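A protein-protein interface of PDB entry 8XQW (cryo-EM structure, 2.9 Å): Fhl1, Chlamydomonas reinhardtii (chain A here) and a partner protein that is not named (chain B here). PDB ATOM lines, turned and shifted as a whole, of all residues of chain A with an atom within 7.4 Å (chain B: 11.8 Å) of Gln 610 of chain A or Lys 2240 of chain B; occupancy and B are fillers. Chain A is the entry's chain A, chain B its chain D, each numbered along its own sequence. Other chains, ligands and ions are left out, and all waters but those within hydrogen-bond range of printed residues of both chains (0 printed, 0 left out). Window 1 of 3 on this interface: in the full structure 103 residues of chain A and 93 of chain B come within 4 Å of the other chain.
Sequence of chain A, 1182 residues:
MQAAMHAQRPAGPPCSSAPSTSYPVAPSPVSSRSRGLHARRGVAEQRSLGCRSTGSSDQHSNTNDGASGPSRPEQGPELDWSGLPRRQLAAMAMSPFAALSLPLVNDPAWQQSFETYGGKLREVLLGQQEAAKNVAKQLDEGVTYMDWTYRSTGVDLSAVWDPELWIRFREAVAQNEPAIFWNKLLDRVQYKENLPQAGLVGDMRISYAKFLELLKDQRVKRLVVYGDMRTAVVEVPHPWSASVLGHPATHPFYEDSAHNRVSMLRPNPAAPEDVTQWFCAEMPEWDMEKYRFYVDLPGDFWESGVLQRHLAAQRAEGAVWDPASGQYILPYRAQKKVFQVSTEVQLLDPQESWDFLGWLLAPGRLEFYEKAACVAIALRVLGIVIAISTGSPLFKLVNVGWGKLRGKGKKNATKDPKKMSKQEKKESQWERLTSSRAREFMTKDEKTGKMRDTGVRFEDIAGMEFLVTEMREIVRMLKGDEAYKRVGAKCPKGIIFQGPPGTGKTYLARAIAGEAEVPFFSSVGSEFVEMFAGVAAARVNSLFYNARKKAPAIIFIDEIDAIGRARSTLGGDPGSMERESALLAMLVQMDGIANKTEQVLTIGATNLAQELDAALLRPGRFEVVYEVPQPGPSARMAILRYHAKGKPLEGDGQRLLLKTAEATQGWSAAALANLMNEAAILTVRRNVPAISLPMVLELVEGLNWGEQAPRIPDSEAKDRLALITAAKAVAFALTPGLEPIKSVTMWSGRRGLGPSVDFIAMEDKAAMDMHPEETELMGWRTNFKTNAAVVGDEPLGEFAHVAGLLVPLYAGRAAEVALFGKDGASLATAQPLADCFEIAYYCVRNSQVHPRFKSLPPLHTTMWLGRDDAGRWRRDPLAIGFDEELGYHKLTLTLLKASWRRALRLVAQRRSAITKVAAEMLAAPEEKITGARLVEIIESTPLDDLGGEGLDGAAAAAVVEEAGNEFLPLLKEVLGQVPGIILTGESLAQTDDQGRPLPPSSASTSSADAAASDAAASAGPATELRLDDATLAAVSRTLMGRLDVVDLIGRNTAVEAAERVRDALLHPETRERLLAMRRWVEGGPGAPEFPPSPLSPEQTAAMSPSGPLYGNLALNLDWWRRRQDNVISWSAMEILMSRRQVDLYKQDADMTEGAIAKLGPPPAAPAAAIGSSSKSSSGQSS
The side-chain amino group of Lys 2240 of chain B sits close to the backbone carbonyl oxygen of Gln 610 of chain A (3.3 Å). The side-chain amino group (NZ) of Lys 2240 of chain B is in hydrogen-bond range of the backbone carbonyl oxygen (O) of Leu 612 of chain A, 3.2 Å away.
The side-chain carboxylate of Glu 611 of chain A sits close to the side-chain amide nitrogen of Gln 610 of chain A (3.1 Å).
Among the printed residues, pairs that only touch across the chains: Gln 498 of chain A with Leu 2239 of chain B (3.8 Å), Ala 609 of chain A with Val 2236 of chain B (3.6 Å) and Gln 610 of chain A with Leu 2239 of chain B (3.2 Å).
Of the printed residues of chain B, Gln 498 of chain A touches Leu 2239 (3.8 Å). Asp 561 of chain A touches none of the printed residues of chain B. No residue of chain B comes within 4 Å of Leu 608 of chain A. Glu 611 of chain A touches none of the printed residues of chain B. Of chain B, only Lys 2240 (3.2 Å) comes within 4 Å of Leu 612 of chain A. Printed residues of chain A within 4 Å of Val 2236 of chain B: Ala 609. Printed residues of chain A within 4 Å of Leu 2239 of chain B: Gln 498 (3.8 Å) and Gln 610 (3.2 Å). Lys 2240 of chain B touches two residues of chain A. The nearest residue of chain B that does not touch Gln 610 of chain A is Lys 2243 of chain B (4.2 Å).
Printed residues of chain A that touch a printed residue of chain B: Gln 498, Ala 609, Gln 610 and Leu 612. Among the printed residues, no Asp or Glu carboxylate lies within 4 Å of a Lys or Arg side-chain nitrogen of the other chain.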
ATOM      1  N   GLN A 498      -4.193 -15.293  30.392  1.00  0.00           N
ATOM      2  CA  GLN A 498      -5.640 -15.208  30.440  1.00  0.00           C
ATOM      3  C   GLN A 498      -6.235 -16.601  30.548  1.00  0.00           C
ATOM      4  O   GLN A 498      -5.675 -17.576  30.041  1.00  0.00           O
ATOM      5  CB  GLN A 498      -6.197 -14.494  29.215  1.00  0.00           C
ATOM      6  CG  GLN A 498      -5.981 -15.242  27.924  1.00  0.00           C
ATOM      7  CD  GLN A 498      -7.283 -15.646  27.275  1.00  0.00           C
ATOM      8  OE1 GLN A 498      -8.360 -15.312  27.765  1.00  0.00           O
ATOM      9  NE2 GLN A 498      -7.194 -16.366  26.166  1.00  0.00           N
ATOM     10  N   ASP A 561      -7.496  -5.806  34.426  1.00  0.00           N
ATOM     11  CA  ASP A 561      -8.863  -5.567  33.975  1.00  0.00           C
ATOM     12  C   ASP A 561      -9.443  -4.297  34.570  1.00  0.00           C
ATOM     13  O   ASP A 561     -10.224  -3.603  33.910  1.00  0.00           O
ATOM     14  CB  ASP A 561      -9.749  -6.755  34.340  1.00  0.00           C
ATOM     15  CG  ASP A 561      -9.314  -8.028  33.663  1.00  0.00           C
ATOM     16  OD1 ASP A 561      -8.963  -7.958  32.468  1.00  0.00           O
ATOM     17  OD2 ASP A 561      -9.299  -9.088  34.329  1.00  0.00           O
ATOM     18  N   ALA A 566     -11.062  -1.312  28.301  1.00  0.00           N
ATOM     19  CA  ALA A 566     -11.266  -0.548  27.080  1.00  0.00           C
ATOM     20  C   ALA A 566     -12.004   0.748  27.383  1.00  0.00           C
ATOM     21  O   ALA A 566     -13.003   0.759  28.107  1.00  0.00           O
ATOM     22  CB  ALA A 566     -12.048  -1.369  26.059  1.00  0.00           C
ATOM     23  N   THR A 606      -5.332 -11.966  33.697  1.00  0.00           N
ATOM     24  CA  THR A 606      -6.731 -11.576  33.633  1.00  0.00           C
ATOM     25  C   THR A 606      -7.599 -12.802  33.414  1.00  0.00           C
ATOM     26  O   THR A 606      -7.160 -13.821  32.878  1.00  0.00           O
ATOM     27  CB  THR A 606      -6.994 -10.576  32.502  1.00  0.00           C
ATOM     28  OG1 THR A 606      -6.587 -11.151  31.256  1.00  0.00           O
ATOM     29  CG2 THR A 606      -6.222  -9.302  32.719  1.00  0.00           C
ATOM     30  N   ASN A 607      -8.856 -12.687  33.838  1.00  0.00           N
ATOM     31  CA  ASN A 607      -9.900 -13.623  33.453  1.00  0.00           C
ATOM     32  C   ASN A 607     -10.989 -12.922  32.654  1.00  0.00           C
ATOM     33  O   ASN A 607     -12.019 -13.537  32.355  1.00  0.00           O
ATOM     34  CB  ASN A 607     -10.500 -14.303  34.684  1.00  0.00           C
ATOM     35  CG  ASN A 607     -10.656 -13.354  35.839  1.00  0.00           C
ATOM     36  OD1 ASN A 607     -10.472 -12.149  35.689  1.00  0.00           O
ATOM     37  ND2 ASN A 607     -10.990 -13.886  37.007  1.00  0.00           N
ATOM     38  N   LEU A 608     -10.777 -11.661  32.299  1.00  0.00           N
ATOM     39  CA  LEU A 608     -11.711 -10.823  31.559  1.00  0.00           C
ATOM     40  C   LEU A 608     -11.031 -10.256  30.327  1.00  0.00           C
ATOM     41  O   LEU A 608     -11.037  -9.050  30.082  1.00  0.00           O
ATOM     42  CB  LEU A 608     -12.242  -9.688  32.425  1.00  0.00           C
ATOM     43  CG  LEU A 608     -13.218 -10.044  33.539  1.00  0.00           C
ATOM     44  CD1 LEU A 608     -13.997  -8.816  33.980  1.00  0.00           C
ATOM     45  CD2 LEU A 608     -14.156 -11.141  33.085  1.00  0.00           C
ATOM     46  N   ALA A 609     -10.403 -11.132  29.542  1.00  0.00           N
ATOM     47  CA  ALA A 609      -9.531 -10.677  28.467  1.00  0.00           C
ATOM     48  C   ALA A 609     -10.251  -9.824  27.432  1.00  0.00           C
ATOM     49  O   ALA A 609      -9.607  -9.009  26.765  1.00  0.00           O
ATOM     50  CB  ALA A 609      -8.875 -11.876  27.789  1.00  0.00           C
ATOM     51  N   GLN A 610     -11.569  -9.976  27.286  1.00  0.00           N
ATOM     52  CA  GLN A 610     -12.274  -9.248  26.236  1.00  0.00           C
ATOM     53  C   GLN A 610     -12.496  -7.786  26.598  1.00  0.00           C
ATOM     54  O   GLN A 610     -12.855  -6.988  25.727  1.00  0.00           O
ATOM     55  CB  GLN A 610     -13.612  -9.919  25.932  1.00  0.00           C
ATOM     56  CG  GLN A 610     -14.611  -9.883  27.072  1.00  0.00           C
ATOM     57  CD  GLN A 610     -14.401 -11.004  28.069  1.00  0.00           C
ATOM     58  OE1 GLN A 610     -13.414 -11.733  28.003  1.00  0.00           O
ATOM     59  NE2 GLN A 610     -15.328 -11.144  29.004  1.00  0.00           N
ATOM     60  N   GLU A 611     -12.303  -7.413  27.858  1.00  0.00           N
ATOM     61  CA  GLU A 611     -12.510  -6.041  28.292  1.00  0.00           C
ATOM     62  C   GLU A 611     -11.296  -5.161  28.048  1.00  0.00           C
ATOM     63  O   GLU A 611     -11.362  -3.950  28.280  1.00  0.00           O
ATOM     64  CB  GLU A 611     -12.887  -6.004  29.770  1.00  0.00           C
ATOM     65  CG  GLU A 611     -14.345  -6.282  30.036  1.00  0.00           C
ATOM     66  CD  GLU A 611     -14.626  -7.756  30.206  1.00  0.00           C
ATOM     67  OE1 GLU A 611     -15.698  -8.101  30.741  1.00  0.00           O
ATOM     68  OE2 GLU A 611     -13.775  -8.569  29.801  1.00  0.00           O
ATOM     69  N   LEU A 612     -10.195  -5.737  27.588  1.00  0.00           N
ATOM     70  CA  LEU A 612      -8.977  -4.975  27.382  1.00  0.00           C
ATOM     71  C   LEU A 612      -9.119  -4.055  26.176  1.00  0.00           C
ATOM     72  O   LEU A 612      -9.770  -4.380  25.182  1.00  0.00           O
ATOM     73  CB  LEU A 612      -7.790  -5.913  27.191  1.00  0.00           C
ATOM     74  CG  LEU A 612      -7.537  -6.917  28.309  1.00  0.00           C
ATOM     75  CD1 LEU A 612      -6.286  -7.714  28.015  1.00  0.00           C
ATOM     76  CD2 LEU A 612      -7.413  -6.203  29.631  1.00  0.00           C
ATOM     77  N   ASP A 613      -8.486  -2.893  26.269  1.00  0.00           N
ATOM     78  CA  ASP A 613      -8.434  -1.946  25.168  1.00  0.00           C
ATOM     79  C   ASP A 613      -7.451  -2.451  24.124  1.00  0.00           C
ATOM     80  O   ASP A 613      -6.365  -2.930  24.463  1.00  0.00           O
ATOM     81  CB  ASP A 613      -8.018  -0.558  25.659  1.00  0.00           C
ATOM     82  CG  ASP A 613      -7.821   0.431  24.527  1.00  0.00           C
ATOM     83  OD1 ASP A 613      -8.437   0.251  23.456  1.00  0.00           O
ATOM     84  OD2 ASP A 613      -7.047   1.390  24.710  1.00  0.00           O
ATOM     85  N   ALA A 614      -7.839  -2.350  22.855  1.00  0.00           N
ATOM     86  CA  ALA A 614      -6.984  -2.842  21.785  1.00  0.00           C
ATOM     87  C   ALA A 614      -5.702  -2.037  21.641  1.00  0.00           C
ATOM     88  O   ALA A 614      -4.786  -2.484  20.942  1.00  0.00           O
ATOM     89  CB  ALA A 614      -7.748  -2.846  20.462  1.00  0.00           C
ATOM     90  N   THR B2231      -0.640 -13.423  17.904  1.00  0.00           N
ATOM     91  CA  THR B2231      -1.410 -14.231  18.838  1.00  0.00           C
ATOM     92  C   THR B2231      -2.362 -13.380  19.645  1.00  0.00           C
ATOM     93  O   THR B2231      -3.422 -13.849  20.059  1.00  0.00           O
ATOM     94  CB  THR B2231      -0.509 -14.999  19.810  1.00  0.00           C
ATOM     95  OG1 THR B2231      -1.324 -15.762  20.705  1.00  0.00           O
ATOM     96  CG2 THR B2231       0.350 -14.052  20.610  1.00  0.00           C
ATOM     97  N   SER B2232      -1.979 -12.121  19.880  1.00  0.00           N
ATOM     98  CA  SER B2232      -2.885 -11.223  20.595  1.00  0.00           C
ATOM     99  C   SER B2232      -4.179 -11.025  19.817  1.00  0.00           C
ATOM    100  O   SER B2232      -5.237 -11.481  20.290  1.00  0.00           O
ATOM    101  CB  SER B2232      -2.170  -9.912  20.932  1.00  0.00           C
ATOM    102  OG  SER B2232      -1.141  -9.611  20.008  1.00  0.00           O
ATOM    103  N   PRO B2233      -4.175 -10.438  18.609  1.00  0.00           N
ATOM    104  CA  PRO B2233      -5.457 -10.130  17.961  1.00  0.00           C
ATOM    105  C   PRO B2233      -6.314 -11.355  17.711  1.00  0.00           C
ATOM    106  O   PRO B2233      -7.509 -11.325  18.013  1.00  0.00           O
ATOM    107  CB  PRO B2233      -5.024  -9.447  16.656  1.00  0.00           C
ATOM    108  CG  PRO B2233      -3.720 -10.045  16.350  1.00  0.00           C
ATOM    109  CD  PRO B2233      -3.046 -10.251  17.677  1.00  0.00           C
ATOM    110  N   PHE B2234      -5.733 -12.440  17.193  1.00  0.00           N
ATOM    111  CA  PHE B2234      -6.491 -13.657  16.924  1.00  0.00           C
ATOM    112  C   PHE B2234      -7.359 -14.025  18.116  1.00  0.00           C
ATOM    113  O   PHE B2234      -8.591 -13.945  18.050  1.00  0.00           O
ATOM    114  CB  PHE B2234      -5.555 -14.830  16.609  1.00  0.00           C
ATOM    115  CG  PHE B2234      -5.545 -15.256  15.164  1.00  0.00           C
ATOM    116  CD1 PHE B2234      -6.700 -15.721  14.553  1.00  0.00           C
ATOM    117  CD2 PHE B2234      -4.377 -15.212  14.426  1.00  0.00           C
ATOM    118  CE1 PHE B2234      -6.687 -16.125  13.234  1.00  0.00           C
ATOM    119  CE2 PHE B2234      -4.357 -15.618  13.109  1.00  0.00           C
ATOM    120  CZ  PHE B2234      -5.518 -16.075  12.511  1.00  0.00           C
ATOM    121  N   SER B2235      -6.718 -14.361  19.233  1.00  0.00           N
ATOM    122  CA  SER B2235      -7.458 -14.894  20.370  1.00  0.00           C
ATOM    123  C   SER B2235      -8.354 -13.831  20.991  1.00  0.00           C
ATOM    124  O   SER B2235      -9.532 -14.092  21.279  1.00  0.00           O
ATOM    125  CB  SER B2235      -6.483 -15.461  21.397  1.00  0.00           C
ATOM    126  OG  SER B2235      -5.816 -16.603  20.879  1.00  0.00           O
ATOM    127  N   VAL B2236      -7.824 -12.620  21.196  1.00  0.00           N
ATOM    128  CA  VAL B2236      -8.588 -11.633  21.951  1.00  0.00           C
ATOM    129  C   VAL B2236      -9.821 -11.203  21.168  1.00  0.00           C
ATOM    130  O   VAL B2236     -10.911 -11.089  21.734  1.00  0.00           O
ATOM    131  CB  VAL B2236      -7.706 -10.432  22.349  1.00  0.00           C
ATOM    132  CG1 VAL B2236      -7.376  -9.556  21.159  1.00  0.00           C
ATOM    133  CG2 VAL B2236      -8.389  -9.610  23.427  1.00  0.00           C
ATOM    134  N   LEU B2237      -9.701 -11.030  19.852  1.00  0.00           N
ATOM    135  CA  LEU B2237     -10.844 -10.576  19.078  1.00  0.00           C
ATOM    136  C   LEU B2237     -11.818 -11.707  18.800  1.00  0.00           C
ATOM    137  O   LEU B2237     -13.031 -11.469  18.756  1.00  0.00           O
ATOM    138  CB  LEU B2237     -10.370  -9.930  17.778  1.00  0.00           C
ATOM    139  CG  LEU B2237      -9.516  -8.676  18.005  1.00  0.00           C
ATOM    140  CD1 LEU B2237      -9.468  -7.791  16.769  1.00  0.00           C
ATOM    141  CD2 LEU B2237     -10.013  -7.881  19.204  1.00  0.00           C
ATOM    142  N   LEU B2238     -11.331 -12.941  18.643  1.00  0.00           N
ATOM    143  CA  LEU B2238     -12.256 -14.060  18.539  1.00  0.00           C
ATOM    144  C   LEU B2238     -13.118 -14.162  19.788  1.00  0.00           C
ATOM    145  O   LEU B2238     -14.351 -14.198  19.704  1.00  0.00           O
ATOM    146  CB  LEU B2238     -11.496 -15.359  18.288  1.00  0.00           C
ATOM    147  CG  LEU B2238     -11.195 -15.722  16.831  1.00  0.00           C
ATOM    148  CD1 LEU B2238     -10.771 -14.526  15.988  1.00  0.00           C
ATOM    149  CD2 LEU B2238     -10.145 -16.816  16.785  1.00  0.00           C
ATOM    150  N   LEU B2239     -12.493 -14.170  20.966  1.00  0.00           N
ATOM    151  CA  LEU B2239     -13.296 -14.291  22.176  1.00  0.00           C
ATOM    152  C   LEU B2239     -14.047 -12.999  22.477  1.00  0.00           C
ATOM    153  O   LEU B2239     -15.006 -13.013  23.253  1.00  0.00           O
ATOM    154  CB  LEU B2239     -12.418 -14.717  23.354  1.00  0.00           C
ATOM    155  CG  LEU B2239     -11.638 -13.703  24.191  1.00  0.00           C
ATOM    156  CD1 LEU B2239     -12.465 -13.200  25.351  1.00  0.00           C
ATOM    157  CD2 LEU B2239     -10.359 -14.327  24.697  1.00  0.00           C
ATOM    158  N   LYS B2240     -13.642 -11.885  21.871  1.00  0.00           N
ATOM    159  CA  LYS B2240     -14.362 -10.636  22.067  1.00  0.00           C
ATOM    160  C   LYS B2240     -15.664 -10.608  21.289  1.00  0.00           C
ATOM    161  O   LYS B2240     -16.691 -10.188  21.830  1.00  0.00           O
ATOM    162  CB  LYS B2240     -13.484  -9.458  21.650  1.00  0.00           C
ATOM    163  CG  LYS B2240     -14.117  -8.100  21.868  1.00  0.00           C
ATOM    164  CD  LYS B2240     -13.084  -6.994  21.733  1.00  0.00           C
ATOM    165  CE  LYS B2240     -13.352  -5.853  22.700  1.00  0.00           C
ATOM    166  NZ  LYS B2240     -12.089  -5.174  23.100  1.00  0.00           N
ATOM    167  N   GLU B2241     -15.641 -11.045  20.033  1.00  0.00           N
ATOM    168  CA  GLU B2241     -16.858 -11.123  19.237  1.00  0.00           C
ATOM    169  C   GLU B2241     -17.667 -12.378  19.521  1.00  0.00           C
ATOM    170  O   GLU B2241     -18.822 -12.458  19.097  1.00  0.00           O
ATOM    171  CB  GLU B2241     -16.527 -11.040  17.741  1.00  0.00           C
ATOM    172  CG  GLU B2241     -15.672 -12.175  17.196  1.00  0.00           C
ATOM    173  CD  GLU B2241     -16.471 -13.406  16.801  1.00  0.00           C
ATOM    174  OE1 GLU B2241     -15.853 -14.464  16.561  1.00  0.00           O
ATOM    175  OE2 GLU B2241     -17.711 -13.313  16.704  1.00  0.00           O
ATOM    176  N   GLU B2242     -17.097 -13.353  20.222  1.00  0.00           N
ATOM    177  CA  GLU B2242     -17.843 -14.542  20.602  1.00  0.00           C
ATOM    178  C   GLU B2242     -18.713 -14.325  21.830  1.00  0.00           C
ATOM    179  O   GLU B2242     -19.755 -14.976  21.959  1.00  0.00           O
ATOM    180  CB  GLU B2242     -16.872 -15.698  20.852  1.00  0.00           C
ATOM    181  CG  GLU B2242     -17.507 -16.960  21.400  1.00  0.00           C
ATOM    182  CD  GLU B2242     -17.399 -17.058  22.907  1.00  0.00           C
ATOM    183  OE1 GLU B2242     -16.299 -17.378  23.405  1.00  0.00           O
ATOM    184  OE2 GLU B2242     -18.411 -16.813  23.594  1.00  0.00           O
ATOM    185  N   LYS B2243     -18.334 -13.412  22.714  1.00  0.00           N
ATOM    186  CA  LYS B2243     -19.029 -13.212  23.975  1.00  0.00           C
ATOM    187  C   LYS B2243     -20.185 -12.225  23.880  1.00  0.00           C
ATOM    188  O   LYS B2243     -20.985 -12.143  24.816  1.00  0.00           O
ATOM    189  CB  LYS B2243     -18.038 -12.732  25.039  1.00  0.00           C
ATOM    190  CG  LYS B2243     -18.432 -13.066  26.464  1.00  0.00           C
ATOM    191  CD  LYS B2243     -18.088 -14.502  26.813  1.00  0.00           C
ATOM    192  CE  LYS B2243     -16.603 -14.670  27.067  1.00  0.00           C
ATOM    193  NZ  LYS B2243     -16.288 -16.056  27.499  1.00  0.00           N
ATOM    194  N   ARG B2244     -20.302 -11.481  22.785  1.00  0.00           N
ATOM    195  CA  ARG B2244     -21.343 -10.474  22.659  1.00  0.00           C
ATOM    196  C   ARG B2244     -22.714 -11.128  22.604  1.00  0.00           C
ATOM    197  O   ARG B2244     -22.843 -12.322  22.322  1.00  0.00           O
ATOM    198  CB  ARG B2244     -21.127  -9.623  21.410  1.00  0.00           C
ATOM    199  CG  ARG B2244     -20.934 -10.442  20.160  1.00  0.00           C
ATOM    200  CD  ARG B2244     -20.585  -9.573  18.969  1.00  0.00           C
ATOM    201  NE  ARG B2244     -21.772  -9.020  18.329  1.00  0.00           N
ATOM    202  CZ  ARG B2244     -22.227  -7.791  18.542  1.00  0.00           C
ATOM    203  NH1 ARG B2244     -21.590  -6.985  19.375  1.00  0.00           N
ATOM    204  NH2 ARG B2244     -23.317  -7.368  17.919  1.00  0.00           N
ATOM    205  N   LEU B2245     -23.743 -10.334  22.881  1.00  0.00           N
ATOM    206  CA  LEU B2245     -25.108 -10.837  22.912  1.00  0.00           C
ATOM    207  C   LEU B2245     -25.661 -10.899  21.498  1.00  0.00           C
ATOM    208  O   LEU B2245     -25.573  -9.923  20.749  1.00  0.00           O
ATOM    209  CB  LEU B2245     -25.984  -9.948  23.783  1.00  0.00           C
ATOM    210  CG  LEU B2245     -27.467 -10.302  23.773  1.00  0.00           C
ATOM    211  CD1 LEU B2245     -27.726 -11.524  24.627  1.00  0.00           C
ATOM    212  CD2 LEU B2245     -28.291  -9.130  24.249  1.00  0.00           C
ATOM    213  N   LYS B2246     -26.231 -12.044  21.134  1.00  0.00           N
ATOM    214  CA  LYS B2246     -26.831 -12.227  19.826  1.00  0.00           C
ATOM    215  C   LYS B2246     -28.320 -12.460  19.984  1.00  0.00           C
ATOM    216  O   LYS B2246     -28.719 -13.499  20.524  1.00  0.00           O
ATOM    217  CB  LYS B2246     -26.182 -13.402  19.110  1.00  0.00           C
ATOM    218  CG  LYS B2246     -24.686 -13.264  18.976  1.00  0.00           C
ATOM    219  CD  LYS B2246     -24.060 -14.533  18.445  1.00  0.00           C
ATOM    220  CE  LYS B2246     -22.714 -14.247  17.810  1.00  0.00           C
ATOM    221  NZ  LYS B2246     -21.792 -13.573  18.759  1.00  0.00           N
ATOM    222  N   ALA B2265     -20.385 -22.320  35.675  1.00  0.00           N
ATOM    223  CA  ALA B2265     -19.921 -20.941  35.700  1.00  0.00           C
ATOM    224  C   ALA B2265     -19.097 -20.580  34.476  1.00  0.00           C
ATOM    225  O   ALA B2265     -18.869 -19.391  34.230  1.00  0.00           O
ATOM    226  CB  ALA B2265     -19.107 -20.682  36.964  1.00  0.00           C
ATOM    227  N   THR B2266     -18.650 -21.565  33.704  1.00  0.00           N
ATOM    228  CA  THR B2266     -17.896 -21.301  32.488  1.00  0.00           C
ATOM    229  C   THR B2266     -18.784 -20.879  31.331  1.00  0.00           C
ATOM    230  O   THR B2266     -18.268 -20.515  30.270  1.00  0.00           O
ATOM    231  CB  THR B2266     -17.092 -22.538  32.086  1.00  0.00           C
ATOM    232  OG1 THR B2266     -17.990 -23.579  31.685  1.00  0.00           O
ATOM    233  CG2 THR B2266     -16.244 -23.022  33.253  1.00  0.00           C
ATOM    234  N   LYS B2267     -20.100 -20.903  31.515  1.00  0.00           N
ATOM    235  CA  LYS B2267     -21.055 -20.636  30.461  1.00  0.00           C
ATOM    236  C   LYS B2267     -21.692 -19.273  30.673  1.00  0.00           C
ATOM    237  O   LYS B2267     -22.077 -18.947  31.803  1.00  0.00           O
ATOM    238  CB  LYS B2267     -22.141 -21.710  30.445  1.00  0.00           C
ATOM    239  CG  LYS B2267     -21.927 -22.802  29.434  1.00  0.00           C
ATOM    240  CD  LYS B2267     -23.047 -23.810  29.510  1.00  0.00           C
ATOM    241  CE  LYS B2267     -22.664 -25.088  28.802  1.00  0.00           C
ATOM    242  NZ  LYS B2267     -21.463 -25.700  29.429  1.00  0.00           N
ATOM    243  N   PRO B2268     -21.820 -18.453  29.634  1.00  0.00           N
ATOM    244  CA  PRO B2268     -22.588 -17.212  29.776  1.00  0.00           C
ATOM    245  C   PRO B2268     -24.041 -17.526  30.086  1.00  0.00           C
ATOM    246  O   PRO B2268     -24.651 -18.394  29.460  1.00  0.00           O
ATOM    247  CB  PRO B2268     -22.424 -16.532  28.415  1.00  0.00           C
ATOM    248  CG  PRO B2268     -22.034 -17.623  27.481  1.00  0.00           C
ATOM    249  CD  PRO B2268     -21.263 -18.617  28.285  1.00  0.00           C
ATOM    250  N   ARG B2269     -24.592 -16.816  31.068  1.00  0.00           N
ATOM    251  CA  ARG B2269     -25.916 -17.155  31.577  1.00  0.00           C
ATOM    252  C   ARG B2269     -26.985 -17.017  30.504  1.00  0.00           C
ATOM    253  O   ARG B2269     -27.955 -17.781  30.479  1.00  0.00           O
ATOM    254  CB  ARG B2269     -26.247 -16.275  32.775  1.00  0.00           C
ATOM    255  CG  ARG B2269     -27.526 -16.658  33.469  1.00  0.00           C
ATOM    256  CD  ARG B2269     -27.370 -16.636  34.972  1.00  0.00           C
ATOM    257  NE  ARG B2269     -28.510 -17.259  35.631  1.00  0.00           N
ATOM    258  CZ  ARG B2269     -28.741 -18.567  35.641  1.00  0.00           C
ATOM    259  NH1 ARG B2269     -27.906 -19.396  35.032  1.00  0.00           N
ATOM    260  NH2 ARG B2269     -29.806 -19.050  36.265  1.00  0.00           N
